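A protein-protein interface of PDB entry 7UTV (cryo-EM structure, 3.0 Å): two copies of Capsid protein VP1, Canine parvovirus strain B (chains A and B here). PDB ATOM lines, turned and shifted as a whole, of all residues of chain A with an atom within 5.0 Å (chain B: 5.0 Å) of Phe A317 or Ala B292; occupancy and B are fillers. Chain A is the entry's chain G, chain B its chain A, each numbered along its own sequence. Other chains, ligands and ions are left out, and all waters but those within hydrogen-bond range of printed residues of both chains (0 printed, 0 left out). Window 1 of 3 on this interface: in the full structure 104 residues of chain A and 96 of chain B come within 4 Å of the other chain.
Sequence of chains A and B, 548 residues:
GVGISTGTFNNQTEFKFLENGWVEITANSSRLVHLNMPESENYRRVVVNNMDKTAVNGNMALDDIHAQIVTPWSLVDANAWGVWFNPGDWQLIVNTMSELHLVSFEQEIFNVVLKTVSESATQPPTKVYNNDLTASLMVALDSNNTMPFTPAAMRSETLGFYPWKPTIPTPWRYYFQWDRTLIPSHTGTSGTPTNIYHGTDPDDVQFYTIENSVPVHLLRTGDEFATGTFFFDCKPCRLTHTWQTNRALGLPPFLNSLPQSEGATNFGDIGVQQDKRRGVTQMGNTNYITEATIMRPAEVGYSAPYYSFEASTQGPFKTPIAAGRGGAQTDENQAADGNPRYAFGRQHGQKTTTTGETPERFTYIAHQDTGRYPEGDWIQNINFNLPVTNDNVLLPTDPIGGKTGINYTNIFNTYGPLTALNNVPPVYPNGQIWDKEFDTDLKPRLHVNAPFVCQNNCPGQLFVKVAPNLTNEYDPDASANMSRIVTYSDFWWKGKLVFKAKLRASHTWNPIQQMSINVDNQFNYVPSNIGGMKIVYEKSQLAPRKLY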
ATOM      1  N   ALA A  61     -16.470 -29.787  -7.397  1.00  0.00           N
ATOM      2  CA  ALA A  61     -15.762 -28.517  -7.355  1.00  0.00           C
ATOM      3  C   ALA A  61     -15.925 -27.771  -6.041  1.00  0.00           C
ATOM      4  O   ALA A  61     -15.163 -26.831  -5.797  1.00  0.00           O
ATOM      5  CB  ALA A  61     -16.228 -27.625  -8.497  1.00  0.00           C
ATOM      6  N   ASP A  63     -15.126 -28.775  -3.139  1.00  0.00           N
ATOM      7  CA  ASP A  63     -14.272 -29.388  -2.139  1.00  0.00           C
ATOM      8  C   ASP A  63     -13.558 -28.319  -1.327  1.00  0.00           C
ATOM      9  O   ASP A  63     -13.004 -27.373  -1.893  1.00  0.00           O
ATOM     10  CB  ASP A  63     -13.267 -30.305  -2.828  1.00  0.00           C
ATOM     11  CG  ASP A  63     -12.307 -30.938  -1.866  1.00  0.00           C
ATOM     12  OD1 ASP A  63     -12.672 -31.077  -0.689  1.00  0.00           O
ATOM     13  OD2 ASP A  63     -11.180 -31.288  -2.268  1.00  0.00           O
ATOM     14  N   SER A 308     -10.908 -26.881 -16.402  1.00  0.00           N
ATOM     15  CA  SER A 308     -10.258 -28.159 -16.179  1.00  0.00           C
ATOM     16  C   SER A 308      -9.790 -28.202 -14.736  1.00  0.00           C
ATOM     17  O   SER A 308      -9.050 -27.315 -14.300  1.00  0.00           O
ATOM     18  CB  SER A 308      -9.078 -28.329 -17.128  1.00  0.00           C
ATOM     19  OG  SER A 308      -8.300 -29.462 -16.793  1.00  0.00           O
ATOM     20  N   PHE A 309     -10.223 -29.220 -14.007  1.00  0.00           N
ATOM     21  CA  PHE A 309      -9.815 -29.453 -12.634  1.00  0.00           C
ATOM     22  C   PHE A 309      -8.856 -30.628 -12.609  1.00  0.00           C
ATOM     23  O   PHE A 309      -9.154 -31.689 -13.162  1.00  0.00           O
ATOM     24  CB  PHE A 309     -11.027 -29.720 -11.747  1.00  0.00           C
ATOM     25  CG  PHE A 309     -11.874 -28.515 -11.514  1.00  0.00           C
ATOM     26  CD1 PHE A 309     -12.806 -28.130 -12.435  1.00  0.00           C
ATOM     27  CD2 PHE A 309     -11.740 -27.779 -10.370  1.00  0.00           C
ATOM     28  CE1 PHE A 309     -13.583 -27.029 -12.225  1.00  0.00           C
ATOM     29  CE2 PHE A 309     -12.513 -26.681 -10.155  1.00  0.00           C
ATOM     30  CZ  PHE A 309     -13.438 -26.304 -11.085  1.00  0.00           C
ATOM     31  N   GLU A 310      -7.700 -30.418 -11.991  1.00  0.00           N
ATOM     32  CA  GLU A 310      -6.642 -31.404 -11.886  1.00  0.00           C
ATOM     33  C   GLU A 310      -6.406 -31.730 -10.427  1.00  0.00           C
ATOM     34  O   GLU A 310      -6.517 -30.860  -9.563  1.00  0.00           O
ATOM     35  CB  GLU A 310      -5.343 -30.893 -12.484  1.00  0.00           C
ATOM     36  CG  GLU A 310      -5.427 -30.528 -13.934  1.00  0.00           C
ATOM     37  CD  GLU A 310      -4.097 -30.061 -14.481  1.00  0.00           C
ATOM     38  OE1 GLU A 310      -3.076 -30.729 -14.213  1.00  0.00           O
ATOM     39  OE2 GLU A 310      -4.064 -29.018 -15.165  1.00  0.00           O
ATOM     40  N   ALA A 311      -6.055 -32.982 -10.168  1.00  0.00           N
ATOM     41  CA  ALA A 311      -5.892 -33.504  -8.824  1.00  0.00           C
ATOM     42  C   ALA A 311      -4.449 -33.895  -8.566  1.00  0.00           C
ATOM     43  O   ALA A 311      -3.714 -34.289  -9.474  1.00  0.00           O
ATOM     44  CB  ALA A 311      -6.793 -34.720  -8.598  1.00  0.00           C
ATOM     45  N   SER A 312      -4.052 -33.750  -7.312  1.00  0.00           N
ATOM     46  CA  SER A 312      -2.859 -34.375  -6.768  1.00  0.00           C
ATOM     47  C   SER A 312      -3.166 -34.629  -5.295  1.00  0.00           C
ATOM     48  O   SER A 312      -4.340 -34.747  -4.924  1.00  0.00           O
ATOM     49  CB  SER A 312      -1.619 -33.520  -7.068  1.00  0.00           C
ATOM     50  OG  SER A 312      -1.814 -32.187  -6.681  1.00  0.00           O
ATOM     51  N   GLY A 315      -6.043 -32.721  -3.314  1.00  0.00           N
ATOM     52  CA  GLY A 315      -7.375 -32.577  -3.853  1.00  0.00           C
ATOM     53  C   GLY A 315      -7.405 -31.855  -5.181  1.00  0.00           C
ATOM     54  O   GLY A 315      -6.370 -31.458  -5.720  1.00  0.00           O
ATOM     55  N   PRO A 316      -8.590 -31.698  -5.751  1.00  0.00           N
ATOM     56  CA  PRO A 316      -8.703 -31.044  -7.052  1.00  0.00           C
ATOM     57  C   PRO A 316      -8.616 -29.530  -6.983  1.00  0.00           C
ATOM     58  O   PRO A 316      -8.966 -28.908  -5.981  1.00  0.00           O
ATOM     59  CB  PRO A 316     -10.087 -31.483  -7.524  1.00  0.00           C
ATOM     60  CG  PRO A 316     -10.827 -31.665  -6.308  1.00  0.00           C
ATOM     61  CD  PRO A 316      -9.881 -32.264  -5.340  1.00  0.00           C
ATOM     62  N   PHE A 317      -8.151 -28.942  -8.086  1.00  0.00           N
ATOM     63  CA  PHE A 317      -8.036 -27.499  -8.220  1.00  0.00           C
ATOM     64  C   PHE A 317      -8.111 -27.106  -9.686  1.00  0.00           C
ATOM     65  O   PHE A 317      -7.679 -27.856 -10.562  1.00  0.00           O
ATOM     66  CB  PHE A 317      -6.727 -26.987  -7.632  1.00  0.00           C
ATOM     67  CG  PHE A 317      -5.515 -27.451  -8.370  1.00  0.00           C
ATOM     68  CD1 PHE A 317      -4.980 -28.687  -8.125  1.00  0.00           C
ATOM     69  CD2 PHE A 317      -4.883 -26.628  -9.273  1.00  0.00           C
ATOM     70  CE1 PHE A 317      -3.871 -29.113  -8.786  1.00  0.00           C
ATOM     71  CE2 PHE A 317      -3.771 -27.051  -9.943  1.00  0.00           C
ATOM     72  CZ  PHE A 317      -3.257 -28.295  -9.696  1.00  0.00           C
ATOM     73  N   LYS A 318      -8.626 -25.906  -9.943  1.00  0.00           N
ATOM     74  CA  LYS A 318      -8.683 -25.389 -11.304  1.00  0.00           C
ATOM     75  C   LYS A 318      -7.286 -25.075 -11.814  1.00  0.00           C
ATOM     76  O   LYS A 318      -6.462 -24.512 -11.088  1.00  0.00           O
ATOM     77  CB  LYS A 318      -9.560 -24.139 -11.355  1.00  0.00           C
ATOM     78  CG  LYS A 318      -9.480 -23.329 -12.648  1.00  0.00           C
ATOM     79  CD  LYS A 318     -10.513 -22.249 -12.655  1.00  0.00           C
ATOM     80  CE  LYS A 318     -10.243 -21.234 -13.744  1.00  0.00           C
ATOM     81  NZ  LYS A 318     -10.378 -21.793 -15.112  1.00  0.00           N
ATOM     82  N   THR A 319      -7.026 -25.433 -13.060  1.00  0.00           N
ATOM     83  CA  THR A 319      -5.822 -24.978 -13.737  1.00  0.00           C
ATOM     84  C   THR A 319      -5.972 -23.497 -14.090  1.00  0.00           C
ATOM     85  O   THR A 319      -6.938 -23.136 -14.774  1.00  0.00           O
ATOM     86  CB  THR A 319      -5.541 -25.833 -14.981  1.00  0.00           C
ATOM     87  OG1 THR A 319      -4.299 -25.430 -15.562  1.00  0.00           O
ATOM     88  CG2 THR A 319      -6.627 -25.746 -16.053  1.00  0.00           C
ATOM     89  N   THR B 245       0.987 -28.443  -3.058  1.00  0.00           N
ATOM     90  CA  THR B 245       0.124 -28.387  -4.217  1.00  0.00           C
ATOM     91  C   THR B 245      -0.498 -26.993  -4.291  1.00  0.00           C
ATOM     92  O   THR B 245      -0.387 -26.196  -3.355  1.00  0.00           O
ATOM     93  CB  THR B 245      -0.908 -29.515  -4.092  1.00  0.00           C
ATOM     94  OG1 THR B 245      -0.214 -30.768  -4.010  1.00  0.00           O
ATOM     95  CG2 THR B 245      -1.917 -29.606  -5.234  1.00  0.00           C
ATOM     96  N   ASN B 246      -1.094 -26.671  -5.438  1.00  0.00           N
ATOM     97  CA  ASN B 246      -1.914 -25.479  -5.606  1.00  0.00           C
ATOM     98  C   ASN B 246      -2.904 -25.265  -4.480  1.00  0.00           C
ATOM     99  O   ASN B 246      -3.127 -24.130  -4.051  1.00  0.00           O
ATOM    100  CB  ASN B 246      -2.684 -25.554  -6.914  1.00  0.00           C
ATOM    101  CG  ASN B 246      -1.891 -25.024  -8.066  1.00  0.00           C
ATOM    102  OD1 ASN B 246      -0.845 -25.568  -8.404  1.00  0.00           O
ATOM    103  ND2 ASN B 246      -2.386 -23.964  -8.697  1.00  0.00           N
ATOM    104  N   ARG B 247      -3.500 -26.346  -3.990  1.00  0.00           N
ATOM    105  CA  ARG B 247      -4.432 -26.253  -2.881  1.00  0.00           C
ATOM    106  C   ARG B 247      -3.796 -25.725  -1.604  1.00  0.00           C
ATOM    107  O   ARG B 247      -4.527 -25.243  -0.737  1.00  0.00           O
ATOM    108  CB  ARG B 247      -5.054 -27.619  -2.630  1.00  0.00           C
ATOM    109  CG  ARG B 247      -6.086 -28.004  -3.668  1.00  0.00           C
ATOM    110  CD  ARG B 247      -7.428 -27.400  -3.376  1.00  0.00           C
ATOM    111  NE  ARG B 247      -8.042 -28.022  -2.213  1.00  0.00           N
ATOM    112  CZ  ARG B 247      -8.904 -29.029  -2.224  1.00  0.00           C
ATOM    113  NH1 ARG B 247      -9.346 -29.569  -3.347  1.00  0.00           N
ATOM    114  NH2 ARG B 247      -9.331 -29.516  -1.067  1.00  0.00           N
ATOM    115  N   THR B 290     -14.368 -21.470  -3.616  1.00  0.00           N
ATOM    116  CA  THR B 290     -14.041 -22.726  -2.959  1.00  0.00           C
ATOM    117  C   THR B 290     -12.541 -22.921  -3.062  1.00  0.00           C
ATOM    118  O   THR B 290     -11.861 -22.217  -3.808  1.00  0.00           O
ATOM    119  CB  THR B 290     -14.761 -23.920  -3.591  1.00  0.00           C
ATOM    120  OG1 THR B 290     -14.027 -24.366  -4.737  1.00  0.00           O
ATOM    121  CG2 THR B 290     -16.187 -23.548  -4.023  1.00  0.00           C
ATOM    122  N   GLU B 291     -12.016 -23.874  -2.296  1.00  0.00           N
ATOM    123  CA  GLU B 291     -10.585 -24.131  -2.360  1.00  0.00           C
ATOM    124  C   GLU B 291     -10.160 -24.654  -3.721  1.00  0.00           C
ATOM    125  O   GLU B 291      -9.011 -24.448  -4.120  1.00  0.00           O
ATOM    126  CB  GLU B 291     -10.173 -25.119  -1.268  1.00  0.00           C
ATOM    127  CG  GLU B 291     -10.264 -24.573   0.146  1.00  0.00           C
ATOM    128  CD  GLU B 291      -9.284 -23.453   0.404  1.00  0.00           C
ATOM    129  OE1 GLU B 291      -8.068 -23.729   0.485  1.00  0.00           O
ATOM    130  OE2 GLU B 291      -9.730 -22.293   0.495  1.00  0.00           O
ATOM    131  N   ALA B 292     -11.061 -25.300  -4.453  1.00  0.00           N
ATOM    132  CA  ALA B 292     -10.748 -25.725  -5.806  1.00  0.00           C
ATOM    133  C   ALA B 292     -10.753 -24.564  -6.785  1.00  0.00           C
ATOM    134  O   ALA B 292      -9.962 -24.558  -7.733  1.00  0.00           O
ATOM    135  CB  ALA B 292     -11.751 -26.783  -6.261  1.00  0.00           C
ATOM    136  N   THR B 293     -11.616 -23.576  -6.564  1.00  0.00           N
ATOM    137  CA  THR B 293     -11.845 -22.499  -7.511  1.00  0.00           C
ATOM    138  C   THR B 293     -11.080 -21.227  -7.193  1.00  0.00           C
ATOM    139  O   THR B 293     -10.944 -20.379  -8.080  1.00  0.00           O
ATOM    140  CB  THR B 293     -13.329 -22.148  -7.559  1.00  0.00           C
ATOM    141  OG1 THR B 293     -13.748 -21.708  -6.265  1.00  0.00           O
ATOM    142  CG2 THR B 293     -14.154 -23.350  -7.966  1.00  0.00           C
ATOM    143  N   ILE B 294     -10.593 -21.057  -5.967  1.00  0.00           N
ATOM    144  CA  ILE B 294      -9.979 -19.794  -5.601  1.00  0.00           C
ATOM    145  C   ILE B 294      -8.637 -19.665  -6.297  1.00  0.00           C
ATOM    146  O   ILE B 294      -7.892 -20.643  -6.449  1.00  0.00           O
ATOM    147  CB  ILE B 294      -9.842 -19.662  -4.077  1.00  0.00           C
ATOM    148  CG1 ILE B 294      -9.492 -18.219  -3.724  1.00  0.00           C
ATOM    149  CG2 ILE B 294      -8.803 -20.620  -3.527  1.00  0.00           C
ATOM    150  CD1 ILE B 294      -9.434 -17.938  -2.272  1.00  0.00           C
ATOM    151  N   GLU B 299       0.609 -22.728 -11.250  1.00  0.00           N
ATOM    152  CA  GLU B 299       0.360 -24.162 -11.186  1.00  0.00           C
ATOM    153  C   GLU B 299       1.662 -24.889 -10.896  1.00  0.00           C
ATOM    154  O   GLU B 299       2.652 -24.704 -11.610  1.00  0.00           O
ATOM    155  CB  GLU B 299      -0.244 -24.667 -12.489  1.00  0.00           C
ATOM    156  CG  GLU B 299      -0.712 -26.111 -12.410  1.00  0.00           C
ATOM    157  CD  GLU B 299      -1.610 -26.518 -13.563  1.00  0.00           C
ATOM    158  OE1 GLU B 299      -2.377 -25.666 -14.056  1.00  0.00           O
ATOM    159  OE2 GLU B 299      -1.553 -27.695 -13.975  1.00  0.00           O
ATOM    160  N   VAL B 300       1.656 -25.700  -9.846  1.00  0.00           N
ATOM    161  CA  VAL B 300       2.778 -26.568  -9.517  1.00  0.00           C
ATOM    162  C   VAL B 300       2.572 -27.893 -10.236  1.00  0.00           C
ATOM    163  O   VAL B 300       1.568 -28.577 -10.019  1.00  0.00           O
ATOM    164  CB  VAL B 300       2.887 -26.771  -8.002  1.00  0.00           C
ATOM    165  CG1 VAL B 300       4.124 -27.593  -7.642  1.00  0.00           C
ATOM    166  CG2 VAL B 300       2.922 -25.439  -7.290  1.00  0.00           C
ATOM    167  N   ARG B 372       0.833 -35.593 -10.321  1.00  0.00           N
ATOM    168  CA  ARG B 372      -0.600 -35.558 -10.553  1.00  0.00           C
ATOM    169  C   ARG B 372      -1.193 -36.921 -10.256  1.00  0.00           C
ATOM    170  O   ARG B 372      -0.499 -37.939 -10.237  1.00  0.00           O
ATOM    171  CB  ARG B 372      -0.935 -35.172 -11.987  1.00  0.00           C
ATOM    172  CG  ARG B 372      -0.636 -33.743 -12.311  1.00  0.00           C
ATOM    173  CD  ARG B 372      -1.702 -32.828 -11.793  1.00  0.00           C
ATOM    174  NE  ARG B 372      -1.447 -31.449 -12.177  1.00  0.00           N
ATOM    175  CZ  ARG B 372      -0.622 -30.617 -11.558  1.00  0.00           C
ATOM    176  NH1 ARG B 372       0.106 -30.991 -10.516  1.00  0.00           N
ATOM    177  NH2 ARG B 372      -0.512 -29.372 -12.004  1.00  0.00           N
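Among the printed residues, merely in contact across the chains: Phe A317 with Asn B246 (3.3 Å), Ala A311 with Arg B372 (3.4 Å), Ala A61 with Ala B292 (3.4 Å), Pro A316 with Ala B292 (3.5 Å), Gly A315 with Arg B247 (3.5 Å), Phe A317 with Ala B292 (3.5 Å), Asp A63 with Glu B291 (3.7 Å), Phe A317 with Arg B372 (3.7 Å), Asp A63 with Ala B292 (3.8 Å) and Phe A309 with Ala B292 (3.97 Å).
The side-chain hydroxyl of Thr B245 lies close to the side-chain hydroxyl of Ser A312, 3.4 Å away. OE1 of Glu B299 lies within hydrogen-bond range of OG1 of Thr A319. The side-chain hydroxyl (OG1) of Thr B290 is in hydrogen-bond range of the backbone carbonyl oxygen (O) of Ala A61 (2.9 Å). The backbone carbonyl oxygen (O) of Pro A316 sits at hydrogen-bond distance from the guanidinium group (NH1) of Arg B247, 2.7 Å away. The side-chain carboxylate (OE2) of Glu A310 lies close to the side-chain carboxylate (OE2) of Glu B299. The backbone NH (N) of Lys A318 is in hydrogen-bond range of the backbone carbonyl oxygen (O) of Ala B292 (2.9 Å). The side-chain carboxylate (OE1) of Glu A310 lies within salt-bridge range of the guanidinium group (NE) of Arg B372, at 2.7 Å. The guanidinium group (NH1) of Arg B247 lies within salt-bridge range of the side-chain carboxylate (OD2) of Asp A63.
No position is printed for both chains.
Hydrophobic or aromatic side chains of chain A that line the printed part of chain B: Phe A309, Pro A316 and Phe A317.
OD1 of Asn B246 sits at hydrogen-bond distance from N of Val B300 (2.9 Å). OG1 of Thr B290 is in hydrogen-bond range of N of Ala B292, at 3.1 Å. The side-chain hydroxyl (OG1) of Thr B293 is in hydrogen-bond range of the backbone NH (N) of Thr B290, 2.7 Å away. The backbone carbonyl oxygen of Val B300 sits at hydrogen-bond distance from the guanidinium group of Arg B372 (2.9 Å). The side-chain carboxylate of Glu B299 lies within salt-bridge range of the guanidinium group of Arg B372, at 2.8 Å. O of Ser A308 is in hydrogen-bond range of N of Thr A319 (3.0 Å).
Phe A317 touches just these residues of chain B: Asn B246 (3.3 Å), Ala B292 (3.5 Å) and Arg B372 (3.7 Å). Ala B292 touches just these residues of chain A: Ala A61 (3.4 Å), Asp A63 (3.8 Å), Phe A309 (3.97 Å), Pro A316 (3.5 Å), Phe A317 (3.5 Å) and Lys A318 (2.9 Å). Printed residues of chain A within 4 Å of Glu B299: Glu A310 (3.1 Å) and Thr A319 (2.5 Å). Printed residues of chain B within 4 Å of Lys A318: Ala B292. Printed residues of chain B within 4 Å of Ser A312: Thr B245. Of the printed residues of chain B, Gly A315 touches Arg B247. Of the printed residues of chain A, Glu B291 touches Asp A63. The nearest residue of chain B that does not touch Phe A317 is Glu B299 (4.04 Å).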
